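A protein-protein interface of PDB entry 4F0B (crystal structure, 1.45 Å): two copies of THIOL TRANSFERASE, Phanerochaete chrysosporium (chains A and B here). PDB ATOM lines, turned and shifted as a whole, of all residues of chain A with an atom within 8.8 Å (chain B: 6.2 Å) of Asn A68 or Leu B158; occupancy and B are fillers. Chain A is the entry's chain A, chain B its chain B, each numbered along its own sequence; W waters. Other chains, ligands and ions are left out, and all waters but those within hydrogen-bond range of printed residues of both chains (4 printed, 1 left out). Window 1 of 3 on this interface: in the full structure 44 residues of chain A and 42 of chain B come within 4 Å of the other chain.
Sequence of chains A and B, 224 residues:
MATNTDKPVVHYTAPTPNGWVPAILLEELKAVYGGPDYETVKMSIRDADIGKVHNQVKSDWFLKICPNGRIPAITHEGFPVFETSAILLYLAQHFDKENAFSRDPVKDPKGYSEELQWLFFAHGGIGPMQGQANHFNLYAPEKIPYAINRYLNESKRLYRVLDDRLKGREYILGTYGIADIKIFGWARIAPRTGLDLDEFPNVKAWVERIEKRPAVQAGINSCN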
ATOM      1  N   VAL A  57      23.620 -14.713  -8.086  1.00  0.00           N
ATOM      2  CA  VAL A  57      24.737 -13.965  -7.505  1.00  0.00           C
ATOM      3  C   VAL A  57      25.235 -14.397  -6.144  1.00  0.00           C
ATOM      4  O   VAL A  57      26.362 -14.053  -5.795  1.00  0.00           O
ATOM      5  CB  VAL A  57      24.467 -12.440  -7.463  1.00  0.00           C
ATOM      6  CG1 VAL A  57      24.358 -11.890  -8.897  1.00  0.00           C
ATOM      7  CG2 VAL A  57      23.227 -12.134  -6.646  1.00  0.00           C
ATOM      8  N   LYS A  58      24.432 -15.172  -5.391  1.00  0.00           N
ATOM      9  CA  LYS A  58      24.877 -15.636  -4.075  1.00  0.00           C
ATOM     10  C   LYS A  58      25.457 -17.048  -4.109  1.00  0.00           C
ATOM     11  O   LYS A  58      25.832 -17.597  -3.064  1.00  0.00           O
ATOM     12  CB  LYS A  58      23.726 -15.576  -3.069  1.00  0.00           C
ATOM     13  CG  LYS A  58      23.104 -14.164  -2.898  1.00  0.00           C
ATOM     14  CD  LYS A  58      24.194 -13.098  -2.696  1.00  0.00           C
ATOM     15  CE  LYS A  58      23.558 -11.713  -2.465  1.00  0.00           C
ATOM     16  NZ  LYS A  58      24.616 -10.651  -2.371  1.00  0.00           N
ATOM     17  N   SER A  59      25.556 -17.624  -5.307  1.00  0.00           N
ATOM     18  CA  SER A  59      26.099 -18.976  -5.457  1.00  0.00           C
ATOM     19  C   SER A  59      27.561 -18.971  -5.030  1.00  0.00           C
ATOM     20  O   SER A  59      28.309 -18.041  -5.338  1.00  0.00           O
ATOM     21  CB  SER A  59      25.968 -19.429  -6.902  1.00  0.00           C
ATOM     22  OG  SER A  59      24.610 -19.612  -7.241  1.00  0.00           O
ATOM     23  N   PHE A  62      30.293 -18.246  -7.567  1.00  0.00           N
ATOM     24  CA  PHE A  62      30.419 -16.877  -8.032  1.00  0.00           C
ATOM     25  C   PHE A  62      31.100 -16.005  -7.001  1.00  0.00           C
ATOM     26  O   PHE A  62      31.744 -15.012  -7.355  1.00  0.00           O
ATOM     27  CB  PHE A  62      29.054 -16.321  -8.431  1.00  0.00           C
ATOM     28  CG  PHE A  62      29.118 -14.917  -9.000  1.00  0.00           C
ATOM     29  CD1 PHE A  62      29.738 -14.680 -10.211  1.00  0.00           C
ATOM     30  CD2 PHE A  62      28.519 -13.851  -8.317  1.00  0.00           C
ATOM     31  CE1 PHE A  62      29.777 -13.384 -10.742  1.00  0.00           C
ATOM     32  CE2 PHE A  62      28.541 -12.558  -8.822  1.00  0.00           C
ATOM     33  CZ  PHE A  62      29.180 -12.327 -10.046  1.00  0.00           C
ATOM     34  N   LEU A  63      30.984 -16.361  -5.721  1.00  0.00           N
ATOM     35  CA  LEU A  63      31.617 -15.588  -4.664  1.00  0.00           C
ATOM     36  C   LEU A  63      33.150 -15.610  -4.822  1.00  0.00           C
ATOM     37  O   LEU A  63      33.827 -14.694  -4.356  1.00  0.00           O
ATOM     38  CB  LEU A  63      31.125 -16.077  -3.278  1.00  0.00           C
ATOM     39  CG  LEU A  63      29.620 -15.866  -3.009  1.00  0.00           C
ATOM     40  CD1 LEU A  63      29.207 -16.387  -1.626  1.00  0.00           C
ATOM     41  CD2 LEU A  63      29.272 -14.381  -3.126  1.00  0.00           C
ATOM     42  N   LYS A  64      33.685 -16.618  -5.533  1.00  0.00           N
ATOM     43  CA  LYS A  64      35.118 -16.656  -5.860  1.00  0.00           C
ATOM     44  C   LYS A  64      35.548 -15.593  -6.859  1.00  0.00           C
ATOM     45  O   LYS A  64      36.740 -15.247  -6.958  1.00  0.00           O
ATOM     46  CB  LYS A  64      35.533 -18.030  -6.415  1.00  0.00           C
ATOM     47  CG  LYS A  64      35.461 -19.171  -5.402  1.00  0.00           C
ATOM     48  CD  LYS A  64      35.938 -20.485  -6.014  1.00  0.00           C
ATOM     49  CE  LYS A  64      35.811 -21.633  -5.011  1.00  0.00           C
ATOM     50  NZ  LYS A  64      36.350 -22.926  -5.545  1.00  0.00           N
ATOM     51  N   ILE A  65      34.582 -15.073  -7.622  1.00  0.00           N
ATOM     52  CA  ILE A  65      34.840 -14.033  -8.608  1.00  0.00           C
ATOM     53  C   ILE A  65      34.450 -12.693  -8.014  1.00  0.00           C
ATOM     54  O   ILE A  65      35.220 -11.726  -8.094  1.00  0.00           O
ATOM     55  CB  ILE A  65      34.046 -14.311  -9.881  1.00  0.00           C
ATOM     56  CG1 ILE A  65      34.587 -15.597 -10.536  1.00  0.00           C
ATOM     57  CG2 ILE A  65      34.143 -13.139 -10.871  1.00  0.00           C
ATOM     58  CD1 ILE A  65      33.650 -16.200 -11.612  1.00  0.00           C
ATOM     59  N   CYS A  66      33.276 -12.629  -7.392  1.00  0.00           N
ATOM     60  CA  CYS A  66      32.811 -11.386  -6.759  1.00  0.00           C
ATOM     61  C   CYS A  66      32.431 -11.680  -5.315  1.00  0.00           C
ATOM     62  O   CYS A  66      31.357 -12.226  -5.057  1.00  0.00           O
ATOM     63  CB  CYS A  66      31.592 -10.807  -7.463  1.00  0.00           C
ATOM     64  SG  CYS A  66      31.030  -9.281  -6.668  1.00  0.00           S
ATOM     65  N   PRO A  67      33.304 -11.341  -4.367  1.00  0.00           N
ATOM     66  CA  PRO A  67      33.017 -11.714  -2.961  1.00  0.00           C
ATOM     67  C   PRO A  67      31.782 -11.023  -2.390  1.00  0.00           C
ATOM     68  O   PRO A  67      31.220 -11.500  -1.402  1.00  0.00           O
ATOM     69  CB  PRO A  67      34.287 -11.316  -2.205  1.00  0.00           C
ATOM     70  CG  PRO A  67      35.063 -10.430  -3.128  1.00  0.00           C
ATOM     71  CD  PRO A  67      34.637 -10.746  -4.559  1.00  0.00           C
ATOM     72  N   ASN A  68      31.345  -9.932  -3.017  1.00  0.00           N
ATOM     73  CA  ASN A  68      30.156  -9.238  -2.612  1.00  0.00           C
ATOM     74  C   ASN A  68      28.871  -9.896  -3.096  1.00  0.00           C
ATOM     75  O   ASN A  68      27.794  -9.500  -2.675  1.00  0.00           O
ATOM     76  CB  ASN A  68      30.230  -7.796  -3.143  1.00  0.00           C
ATOM     77  CG  ASN A  68      29.187  -6.861  -2.527  1.00  0.00           C
ATOM     78  OD1 ASN A  68      28.872  -6.930  -1.334  1.00  0.00           O
ATOM     79  ND2 ASN A  68      28.692  -5.931  -3.338  1.00  0.00           N
ATOM     80  N   GLY A  69      28.974 -10.891  -3.986  1.00  0.00           N
ATOM     81  CA  GLY A  69      27.759 -11.537  -4.471  1.00  0.00           C
ATOM     82  C   GLY A  69      26.817 -10.610  -5.223  1.00  0.00           C
ATOM     83  O   GLY A  69      25.619 -10.616  -4.983  1.00  0.00           O
ATOM     84  N   ARG A  70      27.374  -9.809  -6.135  1.00  0.00           N
ATOM     85  CA  ARG A  70      26.573  -8.875  -6.944  1.00  0.00           C
ATOM     86  C   ARG A  70      27.190  -8.810  -8.344  1.00  0.00           C
ATOM     87  O   ARG A  70      28.372  -9.144  -8.536  1.00  0.00           O
ATOM     88  CB  ARG A  70      26.581  -7.459  -6.351  1.00  0.00           C
ATOM     89  CG  ARG A  70      25.782  -7.352  -5.053  1.00  0.00           C
ATOM     90  CD  ARG A  70      25.275  -5.905  -4.849  1.00  0.00           C
ATOM     91  NE  ARG A  70      24.600  -5.768  -3.594  1.00  0.00           N
ATOM     92  CZ  ARG A  70      24.117  -4.625  -3.152  1.00  0.00           C
ATOM     93  NH1 ARG A  70      24.251  -3.534  -3.894  1.00  0.00           N
ATOM     94  NH2 ARG A  70      23.531  -4.585  -1.948  1.00  0.00           N
ATOM     95  N   ILE A  71      26.367  -8.453  -9.330  1.00  0.00           N
ATOM     96  CA  ILE A  71      26.901  -8.159 -10.668  1.00  0.00           C
ATOM     97  C   ILE A  71      27.116  -6.644 -10.821  1.00  0.00           C
ATOM     98  O   ILE A  71      26.548  -5.833 -10.089  1.00  0.00           O
ATOM     99  CB  ILE A  71      26.003  -8.714 -11.818  1.00  0.00           C
ATOM    100  CG1 ILE A  71      24.573  -8.180 -11.781  1.00  0.00           C
ATOM    101  CG2 ILE A  71      25.986 -10.233 -11.813  1.00  0.00           C
ATOM    102  CD1 ILE A  71      24.413  -6.783 -12.429  1.00  0.00           C
ATOM    103  N   PRO A  72      27.941  -6.232 -11.769  1.00  0.00           N
ATOM    104  CA  PRO A  72      28.730  -7.067 -12.687  1.00  0.00           C
ATOM    105  C   PRO A  72      30.063  -7.466 -12.107  1.00  0.00           C
ATOM    106  O   PRO A  72      30.571  -6.913 -11.119  1.00  0.00           O
ATOM    107  CB  PRO A  72      28.937  -6.138 -13.904  1.00  0.00           C
ATOM    108  CG  PRO A  72      29.041  -4.738 -13.246  1.00  0.00           C
ATOM    109  CD  PRO A  72      28.045  -4.783 -12.079  1.00  0.00           C
ATOM    110  N   ALA A  73      30.634  -8.470 -12.756  1.00  0.00           N
ATOM    111  CA  ALA A  73      32.020  -8.840 -12.535  1.00  0.00           C
ATOM    112  C   ALA A  73      32.553  -9.346 -13.852  1.00  0.00           C
ATOM    113  O   ALA A  73      31.800  -9.794 -14.721  1.00  0.00           O
ATOM    114  CB  ALA A  73      32.162  -9.924 -11.442  1.00  0.00           C
ATOM    115  N   PHE A  82      35.698  -7.155  -9.752  1.00  0.00           N
ATOM    116  CA  PHE A  82      34.326  -6.777  -9.383  1.00  0.00           C
ATOM    117  C   PHE A  82      34.285  -5.274  -9.096  1.00  0.00           C
ATOM    118  O   PHE A  82      35.356  -4.622  -9.009  1.00  0.00           O
ATOM    119  CB  PHE A  82      33.747  -7.653  -8.223  1.00  0.00           C
ATOM    120  CG  PHE A  82      34.364  -7.390  -6.862  1.00  0.00           C
ATOM    121  CD1 PHE A  82      35.622  -7.867  -6.544  1.00  0.00           C
ATOM    122  CD2 PHE A  82      33.645  -6.711  -5.885  1.00  0.00           C
ATOM    123  CE1 PHE A  82      36.190  -7.618  -5.280  1.00  0.00           C
ATOM    124  CE2 PHE A  82      34.209  -6.467  -4.616  1.00  0.00           C
ATOM    125  CZ  PHE A  82      35.468  -6.925  -4.325  1.00  0.00           C
ATOM    126  N   GLU A  83      33.056  -4.750  -9.001  1.00  0.00           N
ATOM    127  CA  GLU A  83      32.691  -3.316  -8.869  1.00  0.00           C
ATOM    128  C   GLU A  83      32.758  -2.610 -10.223  1.00  0.00           C
ATOM    129  O   GLU A  83      33.839  -2.484 -10.825  1.00  0.00           O
ATOM    130  CB  GLU A  83      33.569  -2.566  -7.846  1.00  0.00           C
ATOM    131  CG  GLU A  83      33.424  -3.094  -6.421  1.00  0.00           C
ATOM    132  CD  GLU A  83      32.080  -2.756  -5.785  1.00  0.00           C
ATOM    133  OE1 GLU A  83      31.533  -1.660  -6.082  1.00  0.00           O
ATOM    134  OE2 GLU A  83      31.553  -3.577  -5.012  1.00  0.00           O
ATOM    135  N   THR A  84      31.586  -2.171 -10.699  1.00  0.00           N
ATOM    136  CA  THR A  84      31.468  -1.477 -11.997  1.00  0.00           C
ATOM    137  C   THR A  84      32.681  -0.605 -12.337  1.00  0.00           C
ATOM    138  O   THR A  84      33.332  -0.832 -13.368  1.00  0.00           O
ATOM    139  CB  THR A  84      30.219  -0.542 -12.040  1.00  0.00           C
ATOM    140  OG1 THR A  84      30.209   0.281 -10.866  1.00  0.00           O
ATOM    141  CG2 THR A  84      28.944  -1.362 -12.143  1.00  0.00           C
ATOM    142  N   HIS A 123      30.088   6.467  -7.922  1.00  0.00           N
ATOM    143  CA  HIS A 123      30.073   5.172  -7.252  1.00  0.00           C
ATOM    144  C   HIS A 123      29.584   5.296  -5.792  1.00  0.00           C
ATOM    145  O   HIS A 123      29.009   4.351  -5.241  1.00  0.00           O
ATOM    146  CB  HIS A 123      31.478   4.611  -7.312  1.00  0.00           C
ATOM    147  CG  HIS A 123      31.525   3.133  -7.212  1.00  0.00           C
ATOM    148  ND1 HIS A 123      31.527   2.310  -8.328  1.00  0.00           N
ATOM    149  CD2 HIS A 123      31.604   2.325  -6.129  1.00  0.00           C
ATOM    150  CE1 HIS A 123      31.585   1.050  -7.923  1.00  0.00           C
ATOM    151  NE2 HIS A 123      31.659   1.032  -6.593  1.00  0.00           N
ATOM    152  N   PHE B 121      34.556  -1.167  -3.550  1.00  0.00           N
ATOM    153  CA  PHE B 121      33.631  -1.896  -2.700  1.00  0.00           C
ATOM    154  C   PHE B 121      33.263  -1.080  -1.463  1.00  0.00           C
ATOM    155  O   PHE B 121      32.065  -0.984  -1.106  1.00  0.00           O
ATOM    156  CB  PHE B 121      34.308  -3.201  -2.277  1.00  0.00           C
ATOM    157  CG  PHE B 121      33.593  -3.898  -1.155  1.00  0.00           C
ATOM    158  CD1 PHE B 121      32.395  -4.599  -1.378  1.00  0.00           C
ATOM    159  CD2 PHE B 121      34.128  -3.837   0.121  1.00  0.00           C
ATOM    160  CE1 PHE B 121      31.724  -5.235  -0.283  1.00  0.00           C
ATOM    161  CE2 PHE B 121      33.483  -4.477   1.216  1.00  0.00           C
ATOM    162  CZ  PHE B 121      32.276  -5.188   1.013  1.00  0.00           C
ATOM    163  N   GLY B 125      29.605   0.511  -0.977  1.00  0.00           N
ATOM    164  CA  GLY B 125      28.913  -0.429  -0.094  1.00  0.00           C
ATOM    165  C   GLY B 125      28.973   0.041   1.343  1.00  0.00           C
ATOM    166  O   GLY B 125      27.994   0.630   1.795  1.00  0.00           O
ATOM    167  N   ILE B 126      30.104  -0.146   2.032  1.00  0.00           N
ATOM    168  CA  ILE B 126      30.199   0.197   3.457  1.00  0.00           C
ATOM    169  C   ILE B 126      29.845   1.661   3.720  1.00  0.00           C
ATOM    170  O   ILE B 126      29.000   1.961   4.579  1.00  0.00           O
ATOM    171  CB  ILE B 126      31.562  -0.187   4.015  1.00  0.00           C
ATOM    172  CG1 ILE B 126      31.629  -1.726   4.115  1.00  0.00           C
ATOM    173  CG2 ILE B 126      31.743   0.426   5.414  1.00  0.00           C
ATOM    174  CD1 ILE B 126      32.977  -2.246   4.533  1.00  0.00           C
ATOM    175  N   GLY B 127      30.493   2.608   3.060  1.00  0.00           N
ATOM    176  CA  GLY B 127      30.255   4.030   3.345  1.00  0.00           C
ATOM    177  C   GLY B 127      28.789   4.406   3.136  1.00  0.00           C
ATOM    178  O   GLY B 127      28.119   4.906   4.065  1.00  0.00           O
ATOM    179  N   MET B 129      26.015   2.510   2.834  1.00  0.00           N
ATOM    180  CA  MET B 129      25.008   1.753   3.581  1.00  0.00           C
ATOM    181  C   MET B 129      25.122   2.002   5.067  1.00  0.00           C
ATOM    182  O   MET B 129      24.090   2.141   5.745  1.00  0.00           O
ATOM    183  CB  MET B 129      25.153   0.274   3.222  1.00  0.00           C
ATOM    184  CG  MET B 129      24.838   0.013   1.748  1.00  0.00           C
ATOM    185  SD  MET B 129      23.118   0.409   1.264  1.00  0.00           S
ATOM    186  CE  MET B 129      23.316   2.009   0.478  1.00  0.00           C
ATOM    187  N   GLN B 130      26.335   2.009   5.619  1.00  0.00           N
ATOM    188  CA  GLN B 130      26.500   2.334   7.036  1.00  0.00           C
ATOM    189  C   GLN B 130      26.050   3.767   7.259  1.00  0.00           C
ATOM    190  O   GLN B 130      25.440   4.056   8.296  1.00  0.00           O
ATOM    191  CB  GLN B 130      27.949   2.117   7.491  1.00  0.00           C
ATOM    192  CG  GLN B 130      28.096   2.120   9.016  1.00  0.00           C
ATOM    193  CD  GLN B 130      29.522   1.783   9.422  1.00  0.00           C
ATOM    194  OE1 GLN B 130      30.255   1.190   8.617  1.00  0.00           O
ATOM    195  NE2 GLN B 130      29.954   2.245  10.566  1.00  0.00           N
ATOM    196  N   ASN B 153      20.780  -4.719   8.381  1.00  0.00           N
ATOM    197  CA  ASN B 153      21.052  -6.008   7.711  1.00  0.00           C
ATOM    198  C   ASN B 153      22.081  -5.852   6.605  1.00  0.00           C
ATOM    199  O   ASN B 153      22.987  -6.709   6.460  1.00  0.00           O
ATOM    200  CB  ASN B 153      19.763  -6.581   7.147  1.00  0.00           C
ATOM    201  CG  ASN B 153      18.882  -7.165   8.218  1.00  0.00           C
ATOM    202  OD1 ASN B 153      19.363  -7.600   9.267  1.00  0.00           O
ATOM    203  ND2 ASN B 153      17.584  -7.180   7.973  1.00  0.00           N
ATOM    204  N   GLU B 154      21.999  -4.786   5.810  1.00  0.00           N
ATOM    205  CA  GLU B 154      22.955  -4.630   4.730  1.00  0.00           C
ATOM    206  C   GLU B 154      24.351  -4.349   5.281  1.00  0.00           C
ATOM    207  O   GLU B 154      25.358  -4.869   4.748  1.00  0.00           O
ATOM    208  CB  GLU B 154      22.486  -3.521   3.766  1.00  0.00           C
ATOM    209  CG  GLU B 154      23.487  -3.236   2.639  1.00  0.00           C
ATOM    210  CD  GLU B 154      23.819  -4.423   1.753  1.00  0.00           C
ATOM    211  OE1 GLU B 154      23.167  -5.493   1.814  1.00  0.00           O
ATOM    212  OE2 GLU B 154      24.790  -4.284   0.974  1.00  0.00           O
ATOM    213  N   SER B 155      24.446  -3.528   6.325  1.00  0.00           N
ATOM    214  CA  SER B 155      25.751  -3.286   6.939  1.00  0.00           C
ATOM    215  C   SER B 155      26.344  -4.601   7.482  1.00  0.00           C
ATOM    216  O   SER B 155      27.520  -4.837   7.310  1.00  0.00           O
ATOM    217  CB  SER B 155      25.619  -2.292   8.100  1.00  0.00           C
ATOM    218  OG  SER B 155      25.259  -1.003   7.595  1.00  0.00           O
ATOM    219  N   LYS B 156      25.547  -5.445   8.139  1.00  0.00           N
ATOM    220  CA  LYS B 156      26.025  -6.747   8.602  1.00  0.00           C
ATOM    221  C   LYS B 156      26.542  -7.590   7.430  1.00  0.00           C
ATOM    222  O   LYS B 156      27.587  -8.236   7.563  1.00  0.00           O
ATOM    223  CB  LYS B 156      24.923  -7.490   9.345  1.00  0.00           C
ATOM    224  CG  LYS B 156      24.605  -6.886  10.734  1.00  0.00           C
ATOM    225  CD  LYS B 156      23.326  -7.472  11.266  1.00  0.00           C
ATOM    226  CE  LYS B 156      23.058  -7.007  12.712  1.00  0.00           C
ATOM    227  NZ  LYS B 156      21.752  -7.479  13.225  1.00  0.00           N
ATOM    228  N   ARG B 157      25.816  -7.630   6.310  1.00  0.00           N
ATOM    229  CA  ARG B 157      26.244  -8.403   5.155  1.00  0.00           C
ATOM    230  C   ARG B 157      27.592  -7.906   4.634  1.00  0.00           C
ATOM    231  O   ARG B 157      28.487  -8.731   4.356  1.00  0.00           O
ATOM    232  CB  ARG B 157      25.178  -8.280   4.078  1.00  0.00           C
ATOM    233  CG  ARG B 157      25.423  -9.212   2.898  1.00  0.00           C
ATOM    234  CD  ARG B 157      24.500  -8.861   1.720  1.00  0.00           C
ATOM    235  NE  ARG B 157      24.930  -7.627   1.078  1.00  0.00           N
ATOM    236  CZ  ARG B 157      25.969  -7.523   0.254  1.00  0.00           C
ATOM    237  NH1 ARG B 157      26.710  -8.588  -0.080  1.00  0.00           N
ATOM    238  NH2 ARG B 157      26.277  -6.333  -0.255  1.00  0.00           N
ATOM    239  N   LEU B 158      27.750  -6.592   4.539  1.00  0.00           N
ATOM    240  CA  LEU B 158      29.000  -6.030   4.044  1.00  0.00           C
ATOM    241  C   LEU B 158      30.147  -6.294   5.010  1.00  0.00           C
ATOM    242  O   LEU B 158      31.284  -6.587   4.563  1.00  0.00           O
ATOM    243  CB  LEU B 158      28.853  -4.508   3.843  1.00  0.00           C
ATOM    244  CG  LEU B 158      27.924  -4.150   2.681  1.00  0.00           C
ATOM    245  CD1 LEU B 158      27.495  -2.658   2.833  1.00  0.00           C
ATOM    246  CD2 LEU B 158      28.609  -4.354   1.336  1.00  0.00           C
ATOM    247  N   TYR B 159      29.881  -6.228   6.318  1.00  0.00           N
ATOM    248  CA  TYR B 159      30.945  -6.533   7.297  1.00  0.00           C
ATOM    249  C   TYR B 159      31.322  -8.010   7.279  1.00  0.00           C
ATOM    250  O   TYR B 159      32.477  -8.359   7.573  1.00  0.00           O
ATOM    251  CB  TYR B 159      30.591  -5.991   8.695  1.00  0.00           C
ATOM    252  CG  TYR B 159      31.008  -4.535   8.859  1.00  0.00           C
ATOM    253  CD1 TYR B 159      30.275  -3.501   8.272  1.00  0.00           C
ATOM    254  CD2 TYR B 159      32.139  -4.196   9.579  1.00  0.00           C
ATOM    255  CE1 TYR B 159      30.660  -2.181   8.402  1.00  0.00           C
ATOM    256  CE2 TYR B 159      32.525  -2.876   9.721  1.00  0.00           C
ATOM    257  CZ  TYR B 159      31.803  -1.883   9.095  1.00  0.00           C
ATOM    258  OH  TYR B 159      32.211  -0.582   9.234  1.00  0.00           O
ATOM    259  N   ARG B 160      30.369  -8.876   6.930  1.00  0.00           N
ATOM    260  CA  ARG B 160      30.739 -10.281   6.748  1.00  0.00           C
ATOM    261  C   ARG B 160      31.693 -10.469   5.549  1.00  0.00           C
ATOM    262  O   ARG B 160      32.644 -11.235   5.639  1.00  0.00           O
ATOM    263  CB  ARG B 160      29.504 -11.146   6.585  1.00  0.00           C
ATOM    264  CG  ARG B 160      29.863 -12.614   6.442  1.00  0.00           C
ATOM    265  CD  ARG B 160      30.683 -13.119   7.695  1.00  0.00           C
ATOM    266  NE  ARG B 160      29.936 -13.050   8.967  1.00  0.00           N
ATOM    267  CZ  ARG B 160      30.484 -12.905  10.177  1.00  0.00           C
ATOM    268  NH1 ARG B 160      31.799 -12.816  10.332  1.00  0.00           N
ATOM    269  NH2 ARG B 160      29.696 -12.839  11.242  1.00  0.00           N
ATOM    270  N   VAL B 161      31.418  -9.765   4.457  1.00  0.00           N
ATOM    271  CA  VAL B 161      32.326  -9.823   3.300  1.00  0.00           C
ATOM    272  C   VAL B 161      33.734  -9.358   3.738  1.00  0.00           C
ATOM    273  O   VAL B 161      34.759 -10.017   3.436  1.00  0.00           O
ATOM    274  CB  VAL B 161      31.795  -8.939   2.183  1.00  0.00           C
ATOM    275  CG1 VAL B 161      32.813  -8.838   1.039  1.00  0.00           C
ATOM    276  CG2 VAL B 161      30.471  -9.483   1.661  1.00  0.00           C
ATOM    277  N   LEU B 162      33.787  -8.235   4.462  1.00  0.00           N
ATOM    278  CA  LEU B 162      35.066  -7.740   4.961  1.00  0.00           C
ATOM    279  C   LEU B 162      35.756  -8.718   5.927  1.00  0.00           C
ATOM    280  O   LEU B 162      36.962  -8.977   5.778  1.00  0.00           O
ATOM    281  CB  LEU B 162      34.849  -6.375   5.616  1.00  0.00           C
ATOM    282  CG  LEU B 162      36.118  -5.714   6.140  1.00  0.00           C
ATOM    283  CD1 LEU B 162      37.119  -5.419   4.998  1.00  0.00           C
ATOM    284  CD2 LEU B 162      35.762  -4.449   6.918  1.00  0.00           C
ATOM    285  N   ASP B 163      34.992  -9.287   6.864  1.00  0.00           N
ATOM    286  CA  ASP B 163      35.582 -10.188   7.829  1.00  0.00           C
ATOM    287  C   ASP B 163      36.155 -11.429   7.115  1.00  0.00           C
ATOM    288  O   ASP B 163      37.244 -11.891   7.436  1.00  0.00           O
ATOM    289  CB  ASP B 163      34.539 -10.615   8.857  1.00  0.00           C
ATOM    290  CG  ASP B 163      35.166 -11.280  10.034  1.00  0.00           C
ATOM    291  OD1 ASP B 163      35.243 -12.527  10.037  1.00  0.00           O
ATOM    292  OD2 ASP B 163      35.615 -10.550  10.935  1.00  0.00           O
ATOM    293  N   PHE B 200      32.374  -9.873  14.223  1.00  0.00           N
ATOM    294  CA  PHE B 200      33.270  -9.826  13.054  1.00  0.00           C
ATOM    295  C   PHE B 200      34.705  -9.755  13.583  1.00  0.00           C
ATOM    296  O   PHE B 200      35.347  -8.711  13.503  1.00  0.00           O
ATOM    297  CB  PHE B 200      32.927  -8.596  12.195  1.00  0.00           C
ATOM    298  CG  PHE B 200      31.463  -8.536  11.803  1.00  0.00           C
ATOM    299  CD1 PHE B 200      30.558  -7.759  12.499  1.00  0.00           C
ATOM    300  CD2 PHE B 200      31.012  -9.292  10.748  1.00  0.00           C
ATOM    301  CE1 PHE B 200      29.192  -7.750  12.166  1.00  0.00           C
ATOM    302  CE2 PHE B 200      29.642  -9.292  10.385  1.00  0.00           C
ATOM    303  CZ  PHE B 200      28.727  -8.502  11.116  1.00  0.00           C
HETATM  304  O   HOH W   1      21.814  -6.882  -0.268  1.00  0.00           O
HETATM  305  O   HOH W   2      30.035  -2.180  -3.011  1.00  0.00           O
HETATM  306  O   HOH W   3      26.082 -11.479  -0.047  1.00  0.00           O
HETATM  307  O   HOH W   4      21.890  -2.560  -0.475  1.00  0.00           O
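NH2 of Arg A70 is in salt-bridge range of OE2 of Glu B154, 3.2 Å away. NH2 of Arg B157 is in hydrogen-bond range of OD1 of Asn A68.
The side-chain amino group of Lys A58 is in hydrogen-bond range of the backbone carbonyl oxygen of Asn A68 (3.4 Å). OE1 of Glu A83 lies within hydrogen-bond range of NE2 of His A123 (2.7 Å). SG of Cys A66 sits close to N of Asn A68, at 3.7 Å. SG of Cys A66 lies within hydrogen-bond range of O of Arg A70 (3.3 Å). O of Gly A69 sits at hydrogen-bond distance from NZ of Lys A58 (2.8 Å). OE2 of Glu B154 lies within salt-bridge range of NH2 of Arg B157, 2.8 Å away.
NH1 of Arg B157 touches NZ of Lys A58 (3.7 Å). Pro A67 touches Val B161. Phe B121 touches Asn A68 (CE1 to OD1, 3.5 Å). Asn A68 touches Leu B158 (OD1 to CD2, 3.7 Å). NH2 of Arg A70 touches NH2 of Arg B157 (3.7 Å). Glu A83 touches Phe B121 (OE2 to CA, 3.5 Å).
Printed residues of chain B within 4 Å of Lys A58: Arg B157 (3.7 Å). Asn A68 touches just these residues of chain B: Phe B121, Arg B157 and Leu B158. Printed residues of chain B within 4 Å of Arg A70: Glu B154 (3.2 Å) and Arg B157 (3.7 Å). Of the printed residues of chain B, Glu A83 touches Phe B121. Leu B158 touches just one residue of chain A: Asn A68. Of the printed residues of chain A, Val B161 touches Pro A67 (3.7 Å). The nearest residue of chain A that does not touch Leu B158 is Arg A70 (6.1 Å). The nearest printed residue of chain A that does not touch Val B161 is Asn A68 (4.2 Å).
Printed residues of chain A that touch a printed residue of chain B: Lys A58, Pro A67, Asn A68, Arg A70 and Glu A83. Of the 18 printed residues of chain B, 5 touch a printed residue of chain A. Printed residues of chain B that touch a printed residue of chain A: Phe B121, Glu B154, Arg B157, Leu B158 and Val B161. Among the printed residues, Asp or Glu carboxylates within 4 Å of a Lys or Arg side-chain nitrogen of the other chain: Arg A70 with Glu B154.
No position is printed for both chains. Of the 8 pairs that touch across the chains among the printed residues, none has its exchanged pair printed and touching as well.
Water W1 lies within hydrogen-bond range of OE1 of Glu B154 (2.8 Å), NH2 of Arg A70 (3.3 Å) and NE of Arg B157 (3.5 Å). Water W3 lies within hydrogen-bond range of the side-chain amino group (NZ) of Lys A58 (2.9 Å) and the guanidinium group (NH1) of Arg B157 (3.0 Å). Water W2 lies within hydrogen-bond range of the side-chain carboxylate (OE2) of Glu A83 (2.9 Å), the backbone carbonyl oxygen (O) of Phe B121 (3.0 Å) and the backbone NH (N) of Gly B125 (3.4 Å). Water W4 lies within hydrogen-bond range of NH2 of Arg A70 and SD of Met B129.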
